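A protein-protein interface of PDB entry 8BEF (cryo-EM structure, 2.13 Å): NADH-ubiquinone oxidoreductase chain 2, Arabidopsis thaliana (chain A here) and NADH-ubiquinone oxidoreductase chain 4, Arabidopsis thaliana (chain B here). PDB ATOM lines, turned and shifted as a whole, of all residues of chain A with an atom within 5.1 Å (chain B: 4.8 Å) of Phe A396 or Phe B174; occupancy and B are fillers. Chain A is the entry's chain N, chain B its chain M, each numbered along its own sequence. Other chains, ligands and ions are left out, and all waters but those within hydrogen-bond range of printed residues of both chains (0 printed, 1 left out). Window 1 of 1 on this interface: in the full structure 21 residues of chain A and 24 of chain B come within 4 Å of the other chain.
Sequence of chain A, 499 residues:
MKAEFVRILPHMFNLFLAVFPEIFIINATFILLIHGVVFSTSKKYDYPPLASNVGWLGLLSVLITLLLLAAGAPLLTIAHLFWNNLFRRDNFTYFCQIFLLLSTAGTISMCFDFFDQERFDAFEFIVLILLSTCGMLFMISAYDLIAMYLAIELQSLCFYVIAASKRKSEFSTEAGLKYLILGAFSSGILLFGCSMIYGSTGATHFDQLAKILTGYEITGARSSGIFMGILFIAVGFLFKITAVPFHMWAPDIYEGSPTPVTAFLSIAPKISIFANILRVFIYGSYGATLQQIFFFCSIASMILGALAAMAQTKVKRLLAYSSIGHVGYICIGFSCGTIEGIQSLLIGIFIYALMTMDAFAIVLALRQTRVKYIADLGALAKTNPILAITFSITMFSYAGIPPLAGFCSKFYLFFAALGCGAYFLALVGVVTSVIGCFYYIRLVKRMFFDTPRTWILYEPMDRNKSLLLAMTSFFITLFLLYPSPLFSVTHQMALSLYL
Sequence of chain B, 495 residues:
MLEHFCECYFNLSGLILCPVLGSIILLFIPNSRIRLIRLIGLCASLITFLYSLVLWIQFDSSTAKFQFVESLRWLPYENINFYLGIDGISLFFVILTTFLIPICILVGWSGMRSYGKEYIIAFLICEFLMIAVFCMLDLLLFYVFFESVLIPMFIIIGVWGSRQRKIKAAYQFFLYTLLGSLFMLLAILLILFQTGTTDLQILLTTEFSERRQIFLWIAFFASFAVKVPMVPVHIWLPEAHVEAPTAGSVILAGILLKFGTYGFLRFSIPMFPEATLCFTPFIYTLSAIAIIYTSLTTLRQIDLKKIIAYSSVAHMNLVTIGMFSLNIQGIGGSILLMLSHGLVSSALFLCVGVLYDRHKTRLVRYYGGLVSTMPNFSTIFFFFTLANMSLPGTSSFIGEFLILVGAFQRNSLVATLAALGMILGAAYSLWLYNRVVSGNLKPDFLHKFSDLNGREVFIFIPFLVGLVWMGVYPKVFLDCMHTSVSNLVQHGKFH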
ATOM      1  N   SER A 392     -31.387  13.811 -38.609  1.00  0.00           N
ATOM      2  CA  SER A 392     -30.965  14.063 -37.213  1.00  0.00           C
ATOM      3  C   SER A 392     -30.222  12.840 -36.629  1.00  0.00           C
ATOM      4  O   SER A 392     -29.220  13.034 -36.008  1.00  0.00           O
ATOM      5  CB  SER A 392     -32.173  14.461 -36.384  1.00  0.00           C
ATOM      6  OG  SER A 392     -32.686  15.689 -36.841  1.00  0.00           O
ATOM      7  N   ILE A 393     -30.723  11.651 -36.905  1.00  0.00           N
ATOM      8  CA  ILE A 393     -30.052  10.391 -36.460  1.00  0.00           C
ATOM      9  C   ILE A 393     -28.657  10.330 -37.109  1.00  0.00           C
ATOM     10  O   ILE A 393     -27.709  10.197 -36.375  1.00  0.00           O
ATOM     11  CB  ILE A 393     -30.943   9.184 -36.760  1.00  0.00           C
ATOM     12  CG1 ILE A 393     -32.166   9.109 -35.845  1.00  0.00           C
ATOM     13  CG2 ILE A 393     -30.142   7.890 -36.734  1.00  0.00           C
ATOM     14  CD1 ILE A 393     -33.223   8.182 -36.393  1.00  0.00           C
ATOM     15  N   THR A 394     -28.572  10.537 -38.433  1.00  0.00           N
ATOM     16  CA  THR A 394     -27.261  10.619 -39.122  1.00  0.00           C
ATOM     17  C   THR A 394     -26.323  11.628 -38.397  1.00  0.00           C
ATOM     18  O   THR A 394     -25.265  11.249 -38.081  1.00  0.00           O
ATOM     19  CB  THR A 394     -27.423  10.842 -40.651  1.00  0.00           C
ATOM     20  OG1 THR A 394     -28.597  10.174 -41.117  1.00  0.00           O
ATOM     21  CG2 THR A 394     -26.195  10.478 -41.450  1.00  0.00           C
ATOM     22  N   MET A 395     -26.754  12.862 -38.152  1.00  0.00           N
ATOM     23  CA  MET A 395     -25.948  13.912 -37.454  1.00  0.00           C
ATOM     24  C   MET A 395     -25.514  13.455 -36.053  1.00  0.00           C
ATOM     25  O   MET A 395     -24.382  13.666 -35.689  1.00  0.00           O
ATOM     26  CB  MET A 395     -26.735  15.205 -37.308  1.00  0.00           C
ATOM     27  CG  MET A 395     -27.071  15.884 -38.593  1.00  0.00           C
ATOM     28  SD  MET A 395     -25.591  16.466 -39.394  1.00  0.00           S
ATOM     29  CE  MET A 395     -25.355  15.209 -40.650  1.00  0.00           C
ATOM     30  N   PHE A 396     -26.454  12.902 -35.309  1.00  0.00           N
ATOM     31  CA  PHE A 396     -26.039  12.463 -33.982  1.00  0.00           C
ATOM     32  C   PHE A 396     -25.057  11.304 -34.072  1.00  0.00           C
ATOM     33  O   PHE A 396     -24.146  11.202 -33.244  1.00  0.00           O
ATOM     34  CB  PHE A 396     -27.257  12.078 -33.140  1.00  0.00           C
ATOM     35  CG  PHE A 396     -28.064  13.253 -32.663  1.00  0.00           C
ATOM     36  CD1 PHE A 396     -27.480  14.259 -31.914  1.00  0.00           C
ATOM     37  CD2 PHE A 396     -29.415  13.347 -32.960  1.00  0.00           C
ATOM     38  CE1 PHE A 396     -28.225  15.337 -31.477  1.00  0.00           C
ATOM     39  CE2 PHE A 396     -30.162  14.424 -32.530  1.00  0.00           C
ATOM     40  CZ  PHE A 396     -29.568  15.418 -31.786  1.00  0.00           C
ATOM     41  N   SER A 397     -25.223  10.427 -35.067  1.00  0.00           N
ATOM     42  CA  SER A 397     -24.246   9.370 -35.295  1.00  0.00           C
ATOM     43  C   SER A 397     -22.892   9.943 -35.699  1.00  0.00           C
ATOM     44  O   SER A 397     -21.849   9.482 -35.219  1.00  0.00           O
ATOM     45  CB  SER A 397     -24.760   8.404 -36.361  1.00  0.00           C
ATOM     46  OG  SER A 397     -24.061   7.177 -36.313  1.00  0.00           O
ATOM     47  N   TYR A 398     -22.891  10.947 -36.581  1.00  0.00           N
ATOM     48  CA  TYR A 398     -21.646  11.629 -36.929  1.00  0.00           C
ATOM     49  C   TYR A 398     -20.987  12.223 -35.692  1.00  0.00           C
ATOM     50  O   TYR A 398     -19.762  12.175 -35.546  1.00  0.00           O
ATOM     51  CB  TYR A 398     -21.908  12.733 -37.956  1.00  0.00           C
ATOM     52  CG  TYR A 398     -21.780  12.314 -39.401  1.00  0.00           C
ATOM     53  CD1 TYR A 398     -20.585  11.823 -39.903  1.00  0.00           C
ATOM     54  CD2 TYR A 398     -22.855  12.434 -40.270  1.00  0.00           C
ATOM     55  CE1 TYR A 398     -20.468  11.447 -41.228  1.00  0.00           C
ATOM     56  CE2 TYR A 398     -22.747  12.065 -41.596  1.00  0.00           C
ATOM     57  CZ  TYR A 398     -21.554  11.572 -42.070  1.00  0.00           C
ATOM     58  OH  TYR A 398     -21.447  11.204 -43.387  1.00  0.00           O
ATOM     59  N   ALA A 399     -21.789  12.793 -34.793  1.00  0.00           N
ATOM     60  CA  ALA A 399     -21.260  13.351 -33.557  1.00  0.00           C
ATOM     61  C   ALA A 399     -20.742  12.274 -32.615  1.00  0.00           C
ATOM     62  O   ALA A 399     -19.979  12.587 -31.697  1.00  0.00           O
ATOM     63  CB  ALA A 399     -22.331  14.189 -32.859  1.00  0.00           C
ATOM     64  N   GLY A 400     -21.129  11.020 -32.831  1.00  0.00           N
ATOM     65  CA  GLY A 400     -20.685   9.932 -31.988  1.00  0.00           C
ATOM     66  C   GLY A 400     -21.492   9.725 -30.728  1.00  0.00           C
ATOM     67  O   GLY A 400     -20.999   9.092 -29.792  1.00  0.00           O
ATOM     68  N   ILE A 401     -22.719  10.230 -30.673  1.00  0.00           N
ATOM     69  CA  ILE A 401     -23.552  10.090 -29.482  1.00  0.00           C
ATOM     70  C   ILE A 401     -24.000   8.640 -29.357  1.00  0.00           C
ATOM     71  O   ILE A 401     -24.584   8.086 -30.298  1.00  0.00           O
ATOM     72  CB  ILE A 401     -24.762  11.037 -29.519  1.00  0.00           C
ATOM     73  CG1 ILE A 401     -24.314  12.477 -29.763  1.00  0.00           C
ATOM     74  CG2 ILE A 401     -25.556  10.931 -28.225  1.00  0.00           C
ATOM     75  CD1 ILE A 401     -23.315  12.990 -28.750  1.00  0.00           C
ATOM     76  N   LEU A 404     -25.741   5.218 -30.840  1.00  0.00           N
ATOM     77  CA  LEU A 404     -25.663   5.164 -32.292  1.00  0.00           C
ATOM     78  C   LEU A 404     -24.321   4.591 -32.740  1.00  0.00           C
ATOM     79  O   LEU A 404     -23.331   4.604 -32.004  1.00  0.00           O
ATOM     80  CB  LEU A 404     -25.881   6.550 -32.895  1.00  0.00           C
ATOM     81  CG  LEU A 404     -27.228   7.184 -32.540  1.00  0.00           C
ATOM     82  CD1 LEU A 404     -27.323   8.581 -33.104  1.00  0.00           C
ATOM     83  CD2 LEU A 404     -28.387   6.329 -33.024  1.00  0.00           C
ATOM     84  N   CYS A 437     -19.625  17.914 -32.323  1.00  0.00           N
ATOM     85  CA  CYS A 437     -20.999  17.830 -31.852  1.00  0.00           C
ATOM     86  C   CYS A 437     -21.722  19.153 -32.044  1.00  0.00           C
ATOM     87  O   CYS A 437     -22.893  19.173 -32.439  1.00  0.00           O
ATOM     88  CB  CYS A 437     -21.038  17.409 -30.385  1.00  0.00           C
ATOM     89  SG  CYS A 437     -22.706  17.325 -29.712  1.00  0.00           S
ATOM     90  N   ILE A 441     -25.051  19.331 -34.400  1.00  0.00           N
ATOM     91  CA  ILE A 441     -26.367  19.664 -33.859  1.00  0.00           C
ATOM     92  C   ILE A 441     -26.868  21.016 -34.338  1.00  0.00           C
ATOM     93  O   ILE A 441     -28.057  21.312 -34.175  1.00  0.00           O
ATOM     94  CB  ILE A 441     -26.380  19.628 -32.318  1.00  0.00           C
ATOM     95  CG1 ILE A 441     -25.533  20.759 -31.738  1.00  0.00           C
ATOM     96  CG2 ILE A 441     -25.926  18.263 -31.807  1.00  0.00           C
ATOM     97  CD1 ILE A 441     -25.728  20.952 -30.255  1.00  0.00           C
ATOM     98  N   VAL A 444     -29.472  20.039 -36.781  1.00  0.00           N
ATOM     99  CA  VAL A 444     -30.700  19.634 -36.107  1.00  0.00           C
ATOM    100  C   VAL A 444     -31.468  20.859 -35.630  1.00  0.00           C
ATOM    101  O   VAL A 444     -32.695  20.934 -35.769  1.00  0.00           O
ATOM    102  CB  VAL A 444     -30.386  18.667 -34.950  1.00  0.00           C
ATOM    103  CG1 VAL A 444     -31.668  18.227 -34.265  1.00  0.00           C
ATOM    104  CG2 VAL A 444     -29.608  17.461 -35.467  1.00  0.00           C
ATOM    105  N   LEU B 150     -29.446  13.080 -23.805  1.00  0.00           N
ATOM    106  CA  LEU B 150     -29.130  14.394 -24.353  1.00  0.00           C
ATOM    107  C   LEU B 150     -29.931  14.682 -25.613  1.00  0.00           C
ATOM    108  O   LEU B 150     -30.371  15.812 -25.821  1.00  0.00           O
ATOM    109  CB  LEU B 150     -27.637  14.501 -24.651  1.00  0.00           C
ATOM    110  CG  LEU B 150     -26.777  15.176 -23.590  1.00  0.00           C
ATOM    111  CD1 LEU B 150     -27.160  14.667 -22.212  1.00  0.00           C
ATOM    112  CD2 LEU B 150     -25.309  14.928 -23.880  1.00  0.00           C
ATOM    113  N   ILE B 151     -30.126  13.680 -26.463  1.00  0.00           N
ATOM    114  CA  ILE B 151     -30.813  13.871 -27.740  1.00  0.00           C
ATOM    115  C   ILE B 151     -32.273  14.270 -27.518  1.00  0.00           C
ATOM    116  O   ILE B 151     -32.684  15.348 -27.987  1.00  0.00           O
ATOM    117  CB  ILE B 151     -30.679  12.618 -28.625  1.00  0.00           C
ATOM    118  CG1 ILE B 151     -29.210  12.393 -28.997  1.00  0.00           C
ATOM    119  CG2 ILE B 151     -31.554  12.731 -29.865  1.00  0.00           C
ATOM    120  CD1 ILE B 151     -28.948  11.113 -29.759  1.00  0.00           C
ATOM    121  N   PHE B 154     -32.425  17.732 -25.765  1.00  0.00           N
ATOM    122  CA  PHE B 154     -32.118  18.764 -26.746  1.00  0.00           C
ATOM    123  C   PHE B 154     -33.344  19.094 -27.581  1.00  0.00           C
ATOM    124  O   PHE B 154     -33.704  20.265 -27.746  1.00  0.00           O
ATOM    125  CB  PHE B 154     -30.962  18.277 -27.630  1.00  0.00           C
ATOM    126  CG  PHE B 154     -30.410  19.314 -28.572  1.00  0.00           C
ATOM    127  CD1 PHE B 154     -29.815  20.467 -28.094  1.00  0.00           C
ATOM    128  CD2 PHE B 154     -30.458  19.112 -29.942  1.00  0.00           C
ATOM    129  CE1 PHE B 154     -29.298  21.411 -28.963  1.00  0.00           C
ATOM    130  CE2 PHE B 154     -29.945  20.053 -30.815  1.00  0.00           C
ATOM    131  CZ  PHE B 154     -29.364  21.204 -30.324  1.00  0.00           C
ATOM    132  N   ALA B 170     -30.251  25.400 -25.388  1.00  0.00           N
ATOM    133  CA  ALA B 170     -30.085  24.013 -25.804  1.00  0.00           C
ATOM    134  C   ALA B 170     -28.641  23.714 -26.189  1.00  0.00           C
ATOM    135  O   ALA B 170     -28.098  22.668 -25.804  1.00  0.00           O
ATOM    136  CB  ALA B 170     -31.033  23.703 -26.961  1.00  0.00           C
ATOM    137  N   TYR B 171     -28.007  24.612 -26.953  1.00  0.00           N
ATOM    138  CA  TYR B 171     -26.593  24.433 -27.277  1.00  0.00           C
ATOM    139  C   TYR B 171     -25.760  24.258 -26.011  1.00  0.00           C
ATOM    140  O   TYR B 171     -24.950  23.329 -25.905  1.00  0.00           O
ATOM    141  CB  TYR B 171     -26.064  25.623 -28.081  1.00  0.00           C
ATOM    142  CG  TYR B 171     -26.381  25.624 -29.561  1.00  0.00           C
ATOM    143  CD1 TYR B 171     -26.431  24.444 -30.292  1.00  0.00           C
ATOM    144  CD2 TYR B 171     -26.598  26.819 -30.232  1.00  0.00           C
ATOM    145  CE1 TYR B 171     -26.706  24.458 -31.649  1.00  0.00           C
ATOM    146  CE2 TYR B 171     -26.874  26.843 -31.579  1.00  0.00           C
ATOM    147  CZ  TYR B 171     -26.926  25.664 -32.287  1.00  0.00           C
ATOM    148  OH  TYR B 171     -27.202  25.700 -33.633  1.00  0.00           O
ATOM    149  N   GLN B 172     -25.947  25.156 -25.040  1.00  0.00           N
ATOM    150  CA  GLN B 172     -25.134  25.110 -23.829  1.00  0.00           C
ATOM    151  C   GLN B 172     -25.396  23.844 -23.025  1.00  0.00           C
ATOM    152  O   GLN B 172     -24.451  23.216 -22.529  1.00  0.00           O
ATOM    153  CB  GLN B 172     -25.391  26.347 -22.976  1.00  0.00           C
ATOM    154  CG  GLN B 172     -24.351  27.427 -23.150  1.00  0.00           C
ATOM    155  CD  GLN B 172     -24.817  28.762 -22.628  1.00  0.00           C
ATOM    156  OE1 GLN B 172     -25.005  29.707 -23.390  1.00  0.00           O
ATOM    157  NE2 GLN B 172     -25.017  28.846 -21.321  1.00  0.00           N
ATOM    158  N   PHE B 173     -26.667  23.457 -22.881  1.00  0.00           N
ATOM    159  CA  PHE B 173     -26.990  22.215 -22.188  1.00  0.00           C
ATOM    160  C   PHE B 173     -26.248  21.043 -22.816  1.00  0.00           C
ATOM    161  O   PHE B 173     -25.507  20.315 -22.136  1.00  0.00           O
ATOM    162  CB  PHE B 173     -28.502  21.979 -22.227  1.00  0.00           C
ATOM    163  CG  PHE B 173     -28.916  20.582 -21.850  1.00  0.00           C
ATOM    164  CD1 PHE B 173     -28.917  20.178 -20.526  1.00  0.00           C
ATOM    165  CD2 PHE B 173     -29.289  19.668 -22.823  1.00  0.00           C
ATOM    166  CE1 PHE B 173     -29.296  18.893 -20.177  1.00  0.00           C
ATOM    167  CE2 PHE B 173     -29.667  18.381 -22.480  1.00  0.00           C
ATOM    168  CZ  PHE B 173     -29.669  17.996 -21.152  1.00  0.00           C
ATOM    169  N   PHE B 174     -26.391  20.889 -24.137  1.00  0.00           N
ATOM    170  CA  PHE B 174     -25.789  19.752 -24.821  1.00  0.00           C
ATOM    171  C   PHE B 174     -24.274  19.755 -24.661  1.00  0.00           C
ATOM    172  O   PHE B 174     -23.674  18.727 -24.332  1.00  0.00           O
ATOM    173  CB  PHE B 174     -26.177  19.760 -26.301  1.00  0.00           C
ATOM    174  CG  PHE B 174     -26.200  18.395 -26.936  1.00  0.00           C
ATOM    175  CD1 PHE B 174     -25.062  17.606 -26.976  1.00  0.00           C
ATOM    176  CD2 PHE B 174     -27.363  17.901 -27.497  1.00  0.00           C
ATOM    177  CE1 PHE B 174     -25.087  16.354 -27.557  1.00  0.00           C
ATOM    178  CE2 PHE B 174     -27.394  16.650 -28.080  1.00  0.00           C
ATOM    179  CZ  PHE B 174     -26.254  15.876 -28.113  1.00  0.00           C
ATOM    180  N   LEU B 175     -23.639  20.914 -24.853  1.00  0.00           N
ATOM    181  CA  LEU B 175     -22.180  20.946 -24.892  1.00  0.00           C
ATOM    182  C   LEU B 175     -21.570  20.745 -23.506  1.00  0.00           C
ATOM    183  O   LEU B 175     -20.610  19.978 -23.356  1.00  0.00           O
ATOM    184  CB  LEU B 175     -21.708  22.256 -25.521  1.00  0.00           C
ATOM    185  CG  LEU B 175     -21.978  22.330 -27.028  1.00  0.00           C
ATOM    186  CD1 LEU B 175     -21.861  23.752 -27.553  1.00  0.00           C
ATOM    187  CD2 LEU B 175     -21.049  21.402 -27.788  1.00  0.00           C
ATOM    188  N   TYR B 176     -22.110  21.415 -22.480  1.00  0.00           N
ATOM    189  CA  TYR B 176     -21.629  21.194 -21.118  1.00  0.00           C
ATOM    190  C   TYR B 176     -21.766  19.728 -20.724  1.00  0.00           C
ATOM    191  O   TYR B 176     -20.805  19.100 -20.242  1.00  0.00           O
ATOM    192  CB  TYR B 176     -22.406  22.073 -20.140  1.00  0.00           C
ATOM    193  CG  TYR B 176     -21.760  23.397 -19.813  1.00  0.00           C
ATOM    194  CD1 TYR B 176     -20.853  23.509 -18.768  1.00  0.00           C
ATOM    195  CD2 TYR B 176     -22.073  24.539 -20.534  1.00  0.00           C
ATOM    196  CE1 TYR B 176     -20.268  24.716 -18.458  1.00  0.00           C
ATOM    197  CE2 TYR B 176     -21.495  25.753 -20.233  1.00  0.00           C
ATOM    198  CZ  TYR B 176     -20.593  25.836 -19.193  1.00  0.00           C
ATOM    199  OH  TYR B 176     -20.013  27.043 -18.891  1.00  0.00           O
ATOM    200  N   THR B 177     -22.961  19.162 -20.931  1.00  0.00           N
ATOM    201  CA  THR B 177     -23.192  17.789 -20.505  1.00  0.00           C
ATOM    202  C   THR B 177     -22.302  16.817 -21.268  1.00  0.00           C
ATOM    203  O   THR B 177     -21.777  15.861 -20.684  1.00  0.00           O
ATOM    204  CB  THR B 177     -24.665  17.431 -20.673  1.00  0.00           C
ATOM    205  OG1 THR B 177     -25.477  18.475 -20.123  1.00  0.00           O
ATOM    206  CG2 THR B 177     -24.960  16.155 -19.939  1.00  0.00           C
ATOM    207  N   LEU B 178     -22.098  17.054 -22.567  1.00  0.00           N
ATOM    208  CA  LEU B 178     -21.253  16.160 -23.351  1.00  0.00           C
ATOM    209  C   LEU B 178     -19.795  16.243 -22.917  1.00  0.00           C
ATOM    210  O   LEU B 178     -19.094  15.225 -22.892  1.00  0.00           O
ATOM    211  CB  LEU B 178     -21.394  16.472 -24.840  1.00  0.00           C
ATOM    212  CG  LEU B 178     -20.366  15.785 -25.743  1.00  0.00           C
ATOM    213  CD1 LEU B 178     -20.740  14.331 -25.972  1.00  0.00           C
ATOM    214  CD2 LEU B 178     -20.222  16.518 -27.057  1.00  0.00           C
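The backbone carbonyl oxygen (O) of Phe A396 sits at hydrogen-bond distance from the backbone NH (N) of Ile A401 (3.1 Å).
Among the printed residues, merely in contact across the chains: Cys A437 with Phe B174, Phe A396 with Ile B151, Cys A437 with Leu B178, Ile A441 with Tyr B171, Ile A441 with Phe B154, Ile A401 with Ile B151, Phe A396 with Phe B174 and Ile A401 with Phe B174.
Phe A396 touches just these residues of chain B: Ile B151 (3.5 Å) and Phe B174 (3.7 Å). Printed residues of chain A within 4 Å of Phe B174: Phe A396, Ile A401 and Cys A437. Of the printed residues of chain A, Phe B154 touches Ile A441. Of the printed residues of chain A, Ile B151 touches Phe A396 (3.5 Å) and Ile A401 (3.7 Å). Printed residues of chain A within 4 Å of Leu B178: Cys A437 (3.5 Å). Ser A397 touches none of the printed residues of chain B. Tyr B176 touches none of the printed residues of chain A. The nearest printed residue of chain A that does not touch Phe B174 is Ile A441 (4.2 Å). The nearest printed residue of chain B that does not touch Ile A441 is Phe B174 (4.2 Å).
Hydrophobic or aromatic side chains of chain A within 4 Å of the printed part of chain B: Phe A396, Ile A401 and Ile A441. Printed residues of chain B that touch a printed residue of chain A: Ile B151, Phe B154, Tyr B171, Phe B174 and Leu B178. Hydrophobic or aromatic side chains of chain B within 4 Å of the printed part of chain A: Ile B151, Phe B154, Tyr B171, Phe B174 and Leu B178. Along chain B the printed residues that touch a printed residue of chain A span positions 151 to 178. Among the printed residues, no Asp or Glu carboxylate lies within 4 Å of a Lys or Arg side-chain nitrogen of the other chain.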
